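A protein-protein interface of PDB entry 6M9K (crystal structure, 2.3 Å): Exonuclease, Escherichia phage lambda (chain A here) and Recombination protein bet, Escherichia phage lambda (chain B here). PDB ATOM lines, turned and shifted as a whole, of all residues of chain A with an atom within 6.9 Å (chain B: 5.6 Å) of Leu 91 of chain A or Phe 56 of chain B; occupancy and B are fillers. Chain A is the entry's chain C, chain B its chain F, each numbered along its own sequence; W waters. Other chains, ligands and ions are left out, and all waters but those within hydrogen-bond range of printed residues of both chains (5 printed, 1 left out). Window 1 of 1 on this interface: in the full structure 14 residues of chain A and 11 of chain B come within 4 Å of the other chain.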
ATOM      1  N   TYR A  84      15.289 -20.681   6.339  1.00  0.00           N
ATOM      2  CA  TYR A  84      15.845 -21.196   7.599  1.00  0.00           C
ATOM      3  C   TYR A  84      15.710 -22.695   7.868  1.00  0.00           C
ATOM      4  O   TYR A  84      16.211 -23.164   8.881  1.00  0.00           O
ATOM      5  CB  TYR A  84      15.274 -20.388   8.765  1.00  0.00           C
ATOM      6  CG  TYR A  84      15.743 -18.956   8.750  1.00  0.00           C
ATOM      7  CD1 TYR A  84      17.067 -18.637   9.029  1.00  0.00           C
ATOM      8  CD2 TYR A  84      14.872 -17.917   8.440  1.00  0.00           C
ATOM      9  CE1 TYR A  84      17.510 -17.329   9.003  1.00  0.00           C
ATOM     10  CE2 TYR A  84      15.310 -16.605   8.405  1.00  0.00           C
ATOM     11  CZ  TYR A  84      16.628 -16.318   8.696  1.00  0.00           C
ATOM     12  OH  TYR A  84      17.057 -15.018   8.689  1.00  0.00           O
ATOM     13  N   ASN A  86      17.214 -25.389   6.499  1.00  0.00           N
ATOM     14  CA  ASN A  86      18.509 -26.086   6.609  1.00  0.00           C
ATOM     15  C   ASN A  86      19.205 -25.805   7.936  1.00  0.00           C
ATOM     16  O   ASN A  86      19.738 -26.719   8.545  1.00  0.00           O
ATOM     17  CB  ASN A  86      19.450 -25.771   5.430  1.00  0.00           C
ATOM     18  CG  ASN A  86      18.997 -26.416   4.115  1.00  0.00           C
ATOM     19  OD1 ASN A  86      18.087 -27.256   4.084  1.00  0.00           O
ATOM     20  ND2 ASN A  86      19.634 -26.012   3.011  1.00  0.00           N
ATOM     21  N   ASP A  87      19.160 -24.554   8.393  1.00  0.00           N
ATOM     22  CA  ASP A  87      19.704 -24.208   9.703  1.00  0.00           C
ATOM     23  C   ASP A  87      18.974 -24.965  10.797  1.00  0.00           C
ATOM     24  O   ASP A  87      19.603 -25.501  11.686  1.00  0.00           O
ATOM     25  CB  ASP A  87      19.660 -22.693   9.960  1.00  0.00           C
ATOM     26  CG  ASP A  87      20.658 -21.917   9.105  1.00  0.00           C
ATOM     27  OD1 ASP A  87      21.539 -22.520   8.495  1.00  0.00           O
ATOM     28  OD2 ASP A  87      20.554 -20.686   9.027  1.00  0.00           O
ATOM     29  N   ALA A  88      17.652 -25.036  10.712  1.00  0.00           N
ATOM     30  CA  ALA A  88      16.876 -25.818  11.666  1.00  0.00           C
ATOM     31  C   ALA A  88      17.254 -27.302  11.657  1.00  0.00           C
ATOM     32  O   ALA A  88      17.283 -27.923  12.712  1.00  0.00           O
ATOM     33  CB  ALA A  88      15.390 -25.651  11.413  1.00  0.00           C
ATOM     34  N   ARG A  89      17.532 -27.874  10.485  1.00  0.00           N
ATOM     35  CA  ARG A  89      17.916 -29.285  10.416  1.00  0.00           C
ATOM     36  C   ARG A  89      19.270 -29.488  11.084  1.00  0.00           C
ATOM     37  O   ARG A  89      19.417 -30.355  11.938  1.00  0.00           O
ATOM     38  CB  ARG A  89      17.927 -29.805   8.977  1.00  0.00           C
ATOM     39  CG  ARG A  89      18.037 -31.333   8.859  1.00  0.00           C
ATOM     40  CD  ARG A  89      17.516 -31.899   7.530  1.00  0.00           C
ATOM     41  NE  ARG A  89      17.592 -30.867   6.508  1.00  0.00           N
ATOM     42  CZ  ARG A  89      16.577 -30.328   5.831  1.00  0.00           C
ATOM     43  NH1 ARG A  89      15.330 -30.777   5.925  1.00  0.00           N
ATOM     44  NH2 ARG A  89      16.841 -29.343   4.985  1.00  0.00           N
ATOM     45  N   THR A  90      20.234 -28.662  10.706  1.00  0.00           N
ATOM     46  CA  THR A  90      21.569 -28.647  11.317  1.00  0.00           C
ATOM     47  C   THR A  90      21.533 -28.517  12.849  1.00  0.00           C
ATOM     48  O   THR A  90      22.158 -29.320  13.556  1.00  0.00           O
ATOM     49  CB  THR A  90      22.401 -27.497  10.726  1.00  0.00           C
ATOM     50  OG1 THR A  90      22.473 -27.661   9.304  1.00  0.00           O
ATOM     51  CG2 THR A  90      23.802 -27.478  11.297  1.00  0.00           C
ATOM     52  N   LEU A  91      20.793 -27.521  13.348  1.00  0.00           N
ATOM     53  CA  LEU A  91      20.700 -27.275  14.791  1.00  0.00           C
ATOM     54  C   LEU A  91      20.032 -28.417  15.527  1.00  0.00           C
ATOM     55  O   LEU A  91      20.412 -28.728  16.660  1.00  0.00           O
ATOM     56  CB  LEU A  91      19.966 -25.968  15.123  1.00  0.00           C
ATOM     57  CG  LEU A  91      20.705 -24.624  15.274  1.00  0.00           C
ATOM     58  CD1 LEU A  91      22.174 -24.765  15.648  1.00  0.00           C
ATOM     59  CD2 LEU A  91      20.605 -23.782  14.031  1.00  0.00           C
ATOM     60  N   PHE A  92      19.043 -29.037  14.892  1.00  0.00           N
ATOM     61  CA  PHE A  92      18.437 -30.240  15.440  1.00  0.00           C
ATOM     62  C   PHE A  92      19.434 -31.403  15.494  1.00  0.00           C
ATOM     63  O   PHE A  92      19.490 -32.114  16.490  1.00  0.00           O
ATOM     64  CB  PHE A  92      17.202 -30.683  14.656  1.00  0.00           C
ATOM     65  CG  PHE A  92      16.628 -31.956  15.172  1.00  0.00           C
ATOM     66  CD1 PHE A  92      15.788 -31.945  16.266  1.00  0.00           C
ATOM     67  CD2 PHE A  92      17.009 -33.165  14.626  1.00  0.00           C
ATOM     68  CE1 PHE A  92      15.300 -33.123  16.789  1.00  0.00           C
ATOM     69  CE2 PHE A  92      16.520 -34.347  15.135  1.00  0.00           C
ATOM     70  CZ  PHE A  92      15.666 -34.327  16.220  1.00  0.00           C
ATOM     71  N   GLU A  93      20.188 -31.621  14.422  1.00  0.00           N
ATOM     72  CA  GLU A  93      21.241 -32.645  14.458  1.00  0.00           C
ATOM     73  C   GLU A  93      22.206 -32.396  15.624  1.00  0.00           C
ATOM     74  O   GLU A  93      22.494 -33.301  16.412  1.00  0.00           O
ATOM     75  CB  GLU A  93      22.045 -32.678  13.156  1.00  0.00           C
ATOM     76  CG  GLU A  93      21.302 -33.251  11.969  1.00  0.00           C
ATOM     77  CD  GLU A  93      22.221 -33.479  10.786  1.00  0.00           C
ATOM     78  OE1 GLU A  93      23.010 -34.460  10.851  1.00  0.00           O
ATOM     79  OE2 GLU A  93      22.149 -32.682   9.807  1.00  0.00           O
ATOM     80  N   PHE A  94      22.662 -31.149  15.718  1.00  0.00           N
ATOM     81  CA  PHE A  94      23.690 -30.744  16.658  1.00  0.00           C
ATOM     82  C   PHE A  94      23.212 -30.907  18.085  1.00  0.00           C
ATOM     83  O   PHE A  94      23.853 -31.591  18.876  1.00  0.00           O
ATOM     84  CB  PHE A  94      24.094 -29.294  16.386  1.00  0.00           C
ATOM     85  CG  PHE A  94      25.218 -28.797  17.250  1.00  0.00           C
ATOM     86  CD1 PHE A  94      26.527 -29.199  17.005  1.00  0.00           C
ATOM     87  CD2 PHE A  94      24.973 -27.919  18.294  1.00  0.00           C
ATOM     88  CE1 PHE A  94      27.563 -28.736  17.791  1.00  0.00           C
ATOM     89  CE2 PHE A  94      26.007 -27.460  19.088  1.00  0.00           C
ATOM     90  CZ  PHE A  94      27.301 -27.865  18.838  1.00  0.00           C
ATOM     91  N   THR A  95      22.069 -30.312  18.403  1.00  0.00           N
ATOM     92  CA  THR A  95      21.547 -30.367  19.759  1.00  0.00           C
ATOM     93  C   THR A  95      21.037 -31.753  20.158  1.00  0.00           C
ATOM     94  O   THR A  95      21.221 -32.152  21.292  1.00  0.00           O
ATOM     95  CB  THR A  95      20.446 -29.320  19.982  1.00  0.00           C
ATOM     96  OG1 THR A  95      19.410 -29.487  19.015  1.00  0.00           O
ATOM     97  CG2 THR A  95      21.025 -27.910  19.869  1.00  0.00           C
ATOM     98  N   SER A  96      20.418 -32.497  19.240  1.00  0.00           N
ATOM     99  CA  SER A  96      19.803 -33.794  19.583  1.00  0.00           C
ATOM    100  C   SER A  96      20.815 -34.931  19.639  1.00  0.00           C
ATOM    101  O   SER A  96      20.670 -35.858  20.429  1.00  0.00           O
ATOM    102  CB  SER A  96      18.673 -34.155  18.594  1.00  0.00           C
ATOM    103  OG  SER A  96      19.186 -34.526  17.324  1.00  0.00           O
ATOM    104  N   GLY A  97      21.824 -34.853  18.781  1.00  0.00           N
ATOM    105  CA  GLY A  97      22.805 -35.904  18.646  1.00  0.00           C
ATOM    106  C   GLY A  97      22.381 -37.028  17.722  1.00  0.00           C
ATOM    107  O   GLY A  97      23.105 -38.016  17.608  1.00  0.00           O
ATOM    108  N   TYR A 175      12.195 -23.726  15.001  1.00  0.00           N
ATOM    109  CA  TYR A 175      13.400 -22.927  15.017  1.00  0.00           C
ATOM    110  C   TYR A 175      13.054 -21.474  14.752  1.00  0.00           C
ATOM    111  O   TYR A 175      12.286 -21.176  13.831  1.00  0.00           O
ATOM    112  CB  TYR A 175      14.389 -23.391  13.940  1.00  0.00           C
ATOM    113  CG  TYR A 175      15.641 -22.535  13.820  1.00  0.00           C
ATOM    114  CD1 TYR A 175      16.397 -22.205  14.944  1.00  0.00           C
ATOM    115  CD2 TYR A 175      16.092 -22.078  12.576  1.00  0.00           C
ATOM    116  CE1 TYR A 175      17.552 -21.446  14.837  1.00  0.00           C
ATOM    117  CE2 TYR A 175      17.252 -21.306  12.464  1.00  0.00           C
ATOM    118  CZ  TYR A 175      17.972 -21.000  13.601  1.00  0.00           C
ATOM    119  OH  TYR A 175      19.104 -20.245  13.514  1.00  0.00           O
ATOM    120  N   ASP A 176      13.639 -20.575  15.537  1.00  0.00           N
ATOM    121  CA  ASP A 176      13.490 -19.149  15.309  1.00  0.00           C
ATOM    122  C   ASP A 176      14.846 -18.462  15.464  1.00  0.00           C
ATOM    123  O   ASP A 176      15.316 -18.279  16.576  1.00  0.00           O
ATOM    124  CB  ASP A 176      12.465 -18.556  16.262  1.00  0.00           C
ATOM    125  CG  ASP A 176      12.218 -17.083  16.003  1.00  0.00           C
ATOM    126  OD1 ASP A 176      12.963 -16.479  15.208  1.00  0.00           O
ATOM    127  OD2 ASP A 176      11.268 -16.523  16.588  1.00  0.00           O
ATOM    128  N   PRO A 177      15.457 -18.046  14.350  1.00  0.00           N
ATOM    129  CA  PRO A 177      16.756 -17.384  14.397  1.00  0.00           C
ATOM    130  C   PRO A 177      16.783 -16.006  15.068  1.00  0.00           C
ATOM    131  O   PRO A 177      17.879 -15.478  15.279  1.00  0.00           O
ATOM    132  CB  PRO A 177      17.106 -17.215  12.919  1.00  0.00           C
ATOM    133  CG  PRO A 177      15.789 -17.108  12.238  1.00  0.00           C
ATOM    134  CD  PRO A 177      14.934 -18.103  12.971  1.00  0.00           C
ATOM    135  N   MET A 179      15.376 -15.469  18.107  1.00  0.00           N
ATOM    136  CA  MET A 179      15.421 -15.693  19.547  1.00  0.00           C
ATOM    137  C   MET A 179      16.864 -15.602  20.085  1.00  0.00           C
ATOM    138  O   MET A 179      17.770 -16.265  19.571  1.00  0.00           O
ATOM    139  CB  MET A 179      14.815 -17.061  19.883  1.00  0.00           C
ATOM    140  CG  MET A 179      13.294 -17.131  19.770  1.00  0.00           C
ATOM    141  SD  MET A 179      12.467 -16.284  21.127  1.00  0.00           S
ATOM    142  CE  MET A 179      12.767 -17.385  22.507  1.00  0.00           C
ATOM    143  N   ARG A 181      18.124 -16.555  22.977  1.00  0.00           N
ATOM    144  CA  ARG A 181      18.383 -17.906  23.431  1.00  0.00           C
ATOM    145  C   ARG A 181      17.098 -18.699  23.198  1.00  0.00           C
ATOM    146  O   ARG A 181      16.069 -18.116  22.856  1.00  0.00           O
ATOM    147  CB  ARG A 181      18.727 -17.922  24.922  1.00  0.00           C
ATOM    148  CG  ARG A 181      19.838 -16.958  25.315  1.00  0.00           C
ATOM    149  CD  ARG A 181      20.278 -17.158  26.758  1.00  0.00           C
ATOM    150  NE  ARG A 181      19.253 -16.747  27.726  1.00  0.00           N
ATOM    151  CZ  ARG A 181      18.974 -15.485  28.062  1.00  0.00           C
ATOM    152  NH1 ARG A 181      19.615 -14.456  27.493  1.00  0.00           N
ATOM    153  NH2 ARG A 181      18.034 -15.244  28.973  1.00  0.00           N
ATOM    154  N   GLU A 182      17.166 -20.013  23.396  1.00  0.00           N
ATOM    155  CA  GLU A 182      15.994 -20.897  23.387  1.00  0.00           C
ATOM    156  C   GLU A 182      15.273 -20.966  22.031  1.00  0.00           C
ATOM    157  O   GLU A 182      14.105 -21.314  21.974  1.00  0.00           O
ATOM    158  CB  GLU A 182      14.997 -20.507  24.482  1.00  0.00           C
ATOM    159  CG  GLU A 182      15.596 -20.329  25.861  1.00  0.00           C
ATOM    160  CD  GLU A 182      16.208 -21.600  26.412  1.00  0.00           C
ATOM    161  OE1 GLU A 182      15.682 -22.704  26.125  1.00  0.00           O
ATOM    162  OE2 GLU A 182      17.223 -21.494  27.148  1.00  0.00           O
ATOM    163  N   GLY A 183      15.996 -20.687  20.945  1.00  0.00           N
ATOM    164  CA  GLY A 183      15.418 -20.626  19.610  1.00  0.00           C
ATOM    165  C   GLY A 183      15.196 -21.955  18.910  1.00  0.00           C
ATOM    166  O   GLY A 183      14.612 -21.980  17.836  1.00  0.00           O
ATOM    167  N   LEU A 184      15.650 -23.048  19.514  1.00  0.00           N
ATOM    168  CA  LEU A 184      15.497 -24.389  18.973  1.00  0.00           C
ATOM    169  C   LEU A 184      14.853 -25.211  20.071  1.00  0.00           C
ATOM    170  O   LEU A 184      15.419 -25.372  21.146  1.00  0.00           O
ATOM    171  CB  LEU A 184      16.863 -24.957  18.592  1.00  0.00           C
ATOM    172  CG  LEU A 184      16.995 -26.210  17.713  1.00  0.00           C
ATOM    173  CD1 LEU A 184      16.345 -27.429  18.351  1.00  0.00           C
ATOM    174  CD2 LEU A 184      16.439 -25.971  16.321  1.00  0.00           C
ATOM    175  N   TYR A 186      12.285 -28.863  20.479  1.00  0.00           N
ATOM    176  CA  TYR A 186      11.670 -30.007  19.818  1.00  0.00           C
ATOM    177  C   TYR A 186      11.007 -30.939  20.803  1.00  0.00           C
ATOM    178  O   TYR A 186      11.345 -30.941  21.972  1.00  0.00           O
ATOM    179  CB  TYR A 186      12.679 -30.732  18.924  1.00  0.00           C
ATOM    180  CG  TYR A 186      13.827 -31.426  19.624  1.00  0.00           C
ATOM    181  CD1 TYR A 186      13.658 -32.670  20.207  1.00  0.00           C
ATOM    182  CD2 TYR A 186      15.099 -30.865  19.647  1.00  0.00           C
ATOM    183  CE1 TYR A 186      14.707 -33.318  20.826  1.00  0.00           C
ATOM    184  CE2 TYR A 186      16.159 -31.515  20.264  1.00  0.00           C
ATOM    185  CZ  TYR A 186      15.949 -32.741  20.846  1.00  0.00           C
ATOM    186  OH  TYR A 186      16.977 -33.395  21.465  1.00  0.00           O
ATOM    187  N   LEU B  30      29.505 -24.303  12.149  1.00  0.00           N
ATOM    188  CA  LEU B  30      28.121 -24.159  12.590  1.00  0.00           C
ATOM    189  C   LEU B  30      27.718 -22.702  12.534  1.00  0.00           C
ATOM    190  O   LEU B  30      26.754 -22.342  11.860  1.00  0.00           O
ATOM    191  CB  LEU B  30      27.893 -24.696  14.011  1.00  0.00           C
ATOM    192  CG  LEU B  30      26.524 -25.308  14.370  1.00  0.00           C
ATOM    193  CD1 LEU B  30      26.201 -25.084  15.840  1.00  0.00           C
ATOM    194  CD2 LEU B  30      25.359 -24.815  13.524  1.00  0.00           C
ATOM    195  N   ILE B  34      24.879 -20.651  10.169  1.00  0.00           N
ATOM    196  CA  ILE B  34      23.651 -20.081  10.747  1.00  0.00           C
ATOM    197  C   ILE B  34      23.619 -18.551  10.832  1.00  0.00           C
ATOM    198  O   ILE B  34      22.538 -17.969  10.930  1.00  0.00           O
ATOM    199  CB  ILE B  34      23.267 -20.699  12.118  1.00  0.00           C
ATOM    200  CG1 ILE B  34      24.227 -20.265  13.234  1.00  0.00           C
ATOM    201  CG2 ILE B  34      23.185 -22.223  12.011  1.00  0.00           C
ATOM    202  CD1 ILE B  34      23.794 -20.713  14.617  1.00  0.00           C
ATOM    203  N   VAL B  51      25.995 -15.741  22.338  1.00  0.00           N
ATOM    204  CA  VAL B  51      24.944 -16.137  23.272  1.00  0.00           C
ATOM    205  C   VAL B  51      24.048 -17.210  22.663  1.00  0.00           C
ATOM    206  O   VAL B  51      23.585 -18.082  23.376  1.00  0.00           O
ATOM    207  CB  VAL B  51      24.125 -14.918  23.772  1.00  0.00           C
ATOM    208  CG1 VAL B  51      22.923 -15.347  24.609  1.00  0.00           C
ATOM    209  CG2 VAL B  51      25.014 -14.000  24.599  1.00  0.00           C
ATOM    210  N   LYS B  52      23.827 -17.155  21.351  1.00  0.00           N
ATOM    211  CA  LYS B  52      23.045 -18.188  20.640  1.00  0.00           C
ATOM    212  C   LYS B  52      23.812 -19.505  20.507  1.00  0.00           C
ATOM    213  O   LYS B  52      23.268 -20.578  20.775  1.00  0.00           O
ATOM    214  CB  LYS B  52      22.618 -17.715  19.241  1.00  0.00           C
ATOM    215  CG  LYS B  52      21.627 -16.563  19.217  1.00  0.00           C
ATOM    216  CD  LYS B  52      21.335 -16.138  17.779  1.00  0.00           C
ATOM    217  CE  LYS B  52      20.258 -15.066  17.679  1.00  0.00           C
ATOM    218  NZ  LYS B  52      20.646 -13.779  18.325  1.00  0.00           N
ATOM    219  N   ALA B  53      25.063 -19.419  20.072  1.00  0.00           N
ATOM    220  CA  ALA B  53      25.938 -20.593  20.007  1.00  0.00           C
ATOM    221  C   ALA B  53      26.031 -21.309  21.363  1.00  0.00           C
ATOM    222  O   ALA B  53      26.017 -22.546  21.420  1.00  0.00           O
ATOM    223  CB  ALA B  53      27.325 -20.185  19.540  1.00  0.00           C
ATOM    224  N   LEU B  54      26.109 -20.517  22.435  1.00  0.00           N
ATOM    225  CA  LEU B  54      26.257 -21.031  23.785  1.00  0.00           C
ATOM    226  C   LEU B  54      25.010 -21.771  24.181  1.00  0.00           C
ATOM    227  O   LEU B  54      25.074 -22.857  24.748  1.00  0.00           O
ATOM    228  CB  LEU B  54      26.501 -19.899  24.789  1.00  0.00           C
ATOM    229  CG  LEU B  54      26.508 -20.255  26.283  1.00  0.00           C
ATOM    230  CD1 LEU B  54      27.586 -21.280  26.602  1.00  0.00           C
ATOM    231  CD2 LEU B  54      26.687 -19.009  27.143  1.00  0.00           C
ATOM    232  N   GLY B  55      23.868 -21.156  23.913  1.00  0.00           N
ATOM    233  CA  GLY B  55      22.598 -21.792  24.182  1.00  0.00           C
ATOM    234  C   GLY B  55      22.504 -23.154  23.526  1.00  0.00           C
ATOM    235  O   GLY B  55      22.057 -24.099  24.159  1.00  0.00           O
ATOM    236  N   PHE B  56      22.946 -23.265  22.276  1.00  0.00           N
ATOM    237  CA  PHE B  56      22.895 -24.546  21.567  1.00  0.00           C
ATOM    238  C   PHE B  56      23.859 -25.592  22.158  1.00  0.00           C
ATOM    239  O   PHE B  56      23.484 -26.756  22.298  1.00  0.00           O
ATOM    240  CB  PHE B  56      23.148 -24.364  20.059  1.00  0.00           C
ATOM    241  CG  PHE B  56      22.159 -23.451  19.368  1.00  0.00           C
ATOM    242  CD1 PHE B  56      20.783 -23.513  19.651  1.00  0.00           C
ATOM    243  CD2 PHE B  56      22.601 -22.542  18.396  1.00  0.00           C
ATOM    244  CE1 PHE B  56      19.890 -22.664  19.008  1.00  0.00           C
ATOM    245  CE2 PHE B  56      21.713 -21.704  17.742  1.00  0.00           C
ATOM    246  CZ  PHE B  56      20.361 -21.761  18.049  1.00  0.00           C
ATOM    247  N   LEU B  57      25.083 -25.184  22.510  1.00  0.00           N
ATOM    248  CA  LEU B  57      26.031 -26.085  23.202  1.00  0.00           C
ATOM    249  C   LEU B  57      25.449 -26.578  24.508  1.00  0.00           C
ATOM    250  O   LEU B  57      25.561 -27.760  24.823  1.00  0.00           O
ATOM    251  CB  LEU B  57      27.375 -25.390  23.460  1.00  0.00           C
ATOM    252  CG  LEU B  57      28.204 -25.214  22.181  1.00  0.00           C
ATOM    253  CD1 LEU B  57      29.165 -24.041  22.264  1.00  0.00           C
ATOM    254  CD2 LEU B  57      28.956 -26.497  21.847  1.00  0.00           C
ATOM    255  N   LYS B  58      24.822 -25.668  25.256  1.00  0.00           N
ATOM    256  CA  LYS B  58      24.143 -26.022  26.507  1.00  0.00           C
ATOM    257  C   LYS B  58      23.011 -26.999  26.290  1.00  0.00           C
ATOM    258  O   LYS B  58      22.792 -27.882  27.126  1.00  0.00           O
ATOM    259  CB  LYS B  58      23.606 -24.782  27.227  1.00  0.00           C
ATOM    260  CG  LYS B  58      24.707 -23.959  27.859  1.00  0.00           C
ATOM    261  CD  LYS B  58      24.250 -22.588  28.308  1.00  0.00           C
ATOM    262  CE  LYS B  58      23.757 -22.584  29.730  1.00  0.00           C
ATOM    263  NZ  LYS B  58      23.576 -21.171  30.166  1.00  0.00           N
ATOM    264  N   GLN B  59      22.293 -26.844  25.179  1.00  0.00           N
ATOM    265  CA  GLN B  59      21.205 -27.762  24.850  1.00  0.00           C
ATOM    266  C   GLN B  59      21.758 -29.138  24.493  1.00  0.00           C
ATOM    267  O   GLN B  59      21.229 -30.155  24.955  1.00  0.00           O
ATOM    268  CB  GLN B  59      20.337 -27.218  23.710  1.00  0.00           C
ATOM    269  CG  GLN B  59      18.881 -27.652  23.808  1.00  0.00           C
ATOM    270  CD  GLN B  59      18.003 -27.083  22.699  1.00  0.00           C
ATOM    271  OE1 GLN B  59      18.341 -26.083  22.043  1.00  0.00           O
ATOM    272  NE2 GLN B  59      16.865 -27.733  22.482  1.00  0.00           N
ATOM    273  N   LYS B  60      22.820 -29.150  23.689  1.00  0.00           N
ATOM    274  CA  LYS B  60      23.498 -30.379  23.303  1.00  0.00           C
ATOM    275  C   LYS B  60      23.996 -31.141  24.523  1.00  0.00           C
ATOM    276  O   LYS B  60      23.788 -32.355  24.621  1.00  0.00           O
ATOM    277  CB  LYS B  60      24.669 -30.087  22.367  1.00  0.00           C
ATOM    278  CG  LYS B  60      25.317 -31.330  21.762  1.00  0.00           C
ATOM    279  CD  LYS B  60      26.318 -30.938  20.689  1.00  0.00           C
ATOM    280  CE  LYS B  60      27.016 -32.133  20.065  1.00  0.00           C
ATOM    281  NZ  LYS B  60      26.095 -33.233  19.640  1.00  0.00           N
ATOM    282  N   ALA B  61      24.626 -30.423  25.455  1.00  0.00           N
ATOM    283  CA  ALA B  61      25.120 -31.023  26.688  1.00  0.00           C
ATOM    284  C   ALA B  61      23.984 -31.558  27.545  1.00  0.00           C
ATOM    285  O   ALA B  61      24.054 -32.689  28.017  1.00  0.00           O
ATOM    286  CB  ALA B  61      25.947 -30.022  27.484  1.00  0.00           C
HETATM  287  O   HOH W   1      19.805 -19.276  11.170  1.00  0.00           O
HETATM  288  O   HOH W   2      17.776 -23.468  22.139  1.00  0.00           O
HETATM  289  O   HOH W   3      25.250 -34.374  16.656  1.00  0.00           O
HETATM  290  O   HOH W   4      19.466 -21.964  23.598  1.00  0.00           O
HETATM  291  O   HOH W   5      14.223 -29.332  22.660  1.00  0.00           O
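The backbone carbonyl oxygen (O) of Phe 94 of chain A lies within hydrogen-bond range of the side-chain amino group (NZ) of Lys 60 of chain B (2.9 Å). The backbone carbonyl oxygen (O) of Leu 184 of chain A sits at hydrogen-bond distance from the side-chain amide nitrogen (NE2) of Gln 59 of chain B, 3.1 Å away.
Water W1 lies within hydrogen-bond range of OH of Tyr 175 of chain A (2.6 Å), OD2 of Asp 87 of chain A (2.7 Å) and O of Ile 34 of chain B (3.0 Å). Water W2 bridges the side-chain amide oxygen of Gln 59 of chain B (2.7 Å) and the backbone carbonyl oxygen of Leu 184 of chain A (3.2 Å). Water W5 lies within hydrogen-bond range of the backbone NH (N) of Tyr 186 of chain A (3.0 Å) and the side-chain amide nitrogen (NE2) of Gln 59 of chain B (3.1 Å). Water W3 lies within hydrogen-bond range of the backbone carbonyl oxygen (O) of Glu 93 of chain A and the side-chain amino group (NZ) of Lys 60 of chain B. Water W4 bridges the backbone NH of Glu 182 of chain A (3.0 Å) and the backbone carbonyl oxygen of Gly 55 of chain B (3.4 Å).
OG1 of Thr 90 of chain A sits at hydrogen-bond distance from O of Asn 86 of chain A, 3.0 Å away. The backbone carbonyl oxygen (O) of Leu 91 of chain A sits at hydrogen-bond distance from the side-chain hydroxyl (OG1) of Thr 95 of chain A, at 2.7 Å.
Printed residues of chain B that touch a printed residue of chain A: Leu 30, Ile 34, Val 51, Lys 52, Phe 56, Leu 57, Gln 59 and Lys 60. Hydrophobic or aromatic side chains of chain B within 4 Å of the printed part of chain A: Leu 30, Ile 34, Val 51, Phe 56 and Leu 57. Printed residues of chain A that touch a printed residue of chain B: Asp 87, Thr 90, Leu 91, Phe 94, Thr 95, Pro 177, Met 179, Arg 181 and Leu 184. Hydrophobic or aromatic side chains of chain A within 4 Å of the printed part of chain B: Leu 91, Phe 94 and Leu 184. Among the printed residues, no Asp or Glu carboxylate lies within 4 Å of a Lys or Arg side-chain nitrogen of the other chain.
Of the printed residues of chain B, Asp 87 of chain A touches Ile 34 (3.6 Å). Leu 91 of chain A touches just these residues of chain B: Leu 30 (3.8 Å), Ile 34 (3.6 Å) and Phe 56 (3.6 Å). Phe 92 of chain A touches none of the printed residues of chain B. Printed residues of chain B within 4 Å of Leu 184 of chain A: Phe 56 (3.8 Å) and Gln 59 (3.1 Å). Printed residues of chain A within 4 Å of Phe 56 of chain B: Leu 91 (3.6 Å), Thr 95 (3.6 Å) and Leu 184 (3.8 Å). Of the printed residues of chain A, Leu 57 of chain B touches Phe 94 (3.7 Å). The nearest printed residue of chain B that does not touch Leu 91 of chain A is Gln 59 of chain B (6.3 Å). The nearest residue of chain A that does not touch Phe 56 of chain B is Phe 94 of chain A (4.1 Å). The nearest printed residue of chain A that does not touch Lys 60 of chain B is Gly 97 of chain A (4.4 Å).
Ile 34 of chain B touches Asp 87 of chain A. CG2 of Thr 90 of chain A touches CD2 of Leu 30 of chain B, 3.8 Å away. CD1 of Leu 91 of chain A touches CD2 of Leu 30 of chain B, 3.8 Å away. CG2 of Ile 34 of chain B touches CD2 of Leu 91 of chain A (3.6 Å). Phe 56 of chain B touches Leu 91 of chain A (CD2 to CD1, 3.6 Å). Phe 56 of chain B touches Thr 95 of chain A. CE of Lys 52 of chain B touches O of Pro 177 of chain A (3.4 Å). Lys 52 of chain B touches Met 179 of chain A (CE to O, 3.3 Å). CG of Arg 181 of chain A touches CG1 of Val 51 of chain B (3.6 Å). Phe 56 of chain B touches Leu 184 of chain A (CE1 to CB, 3.8 Å).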
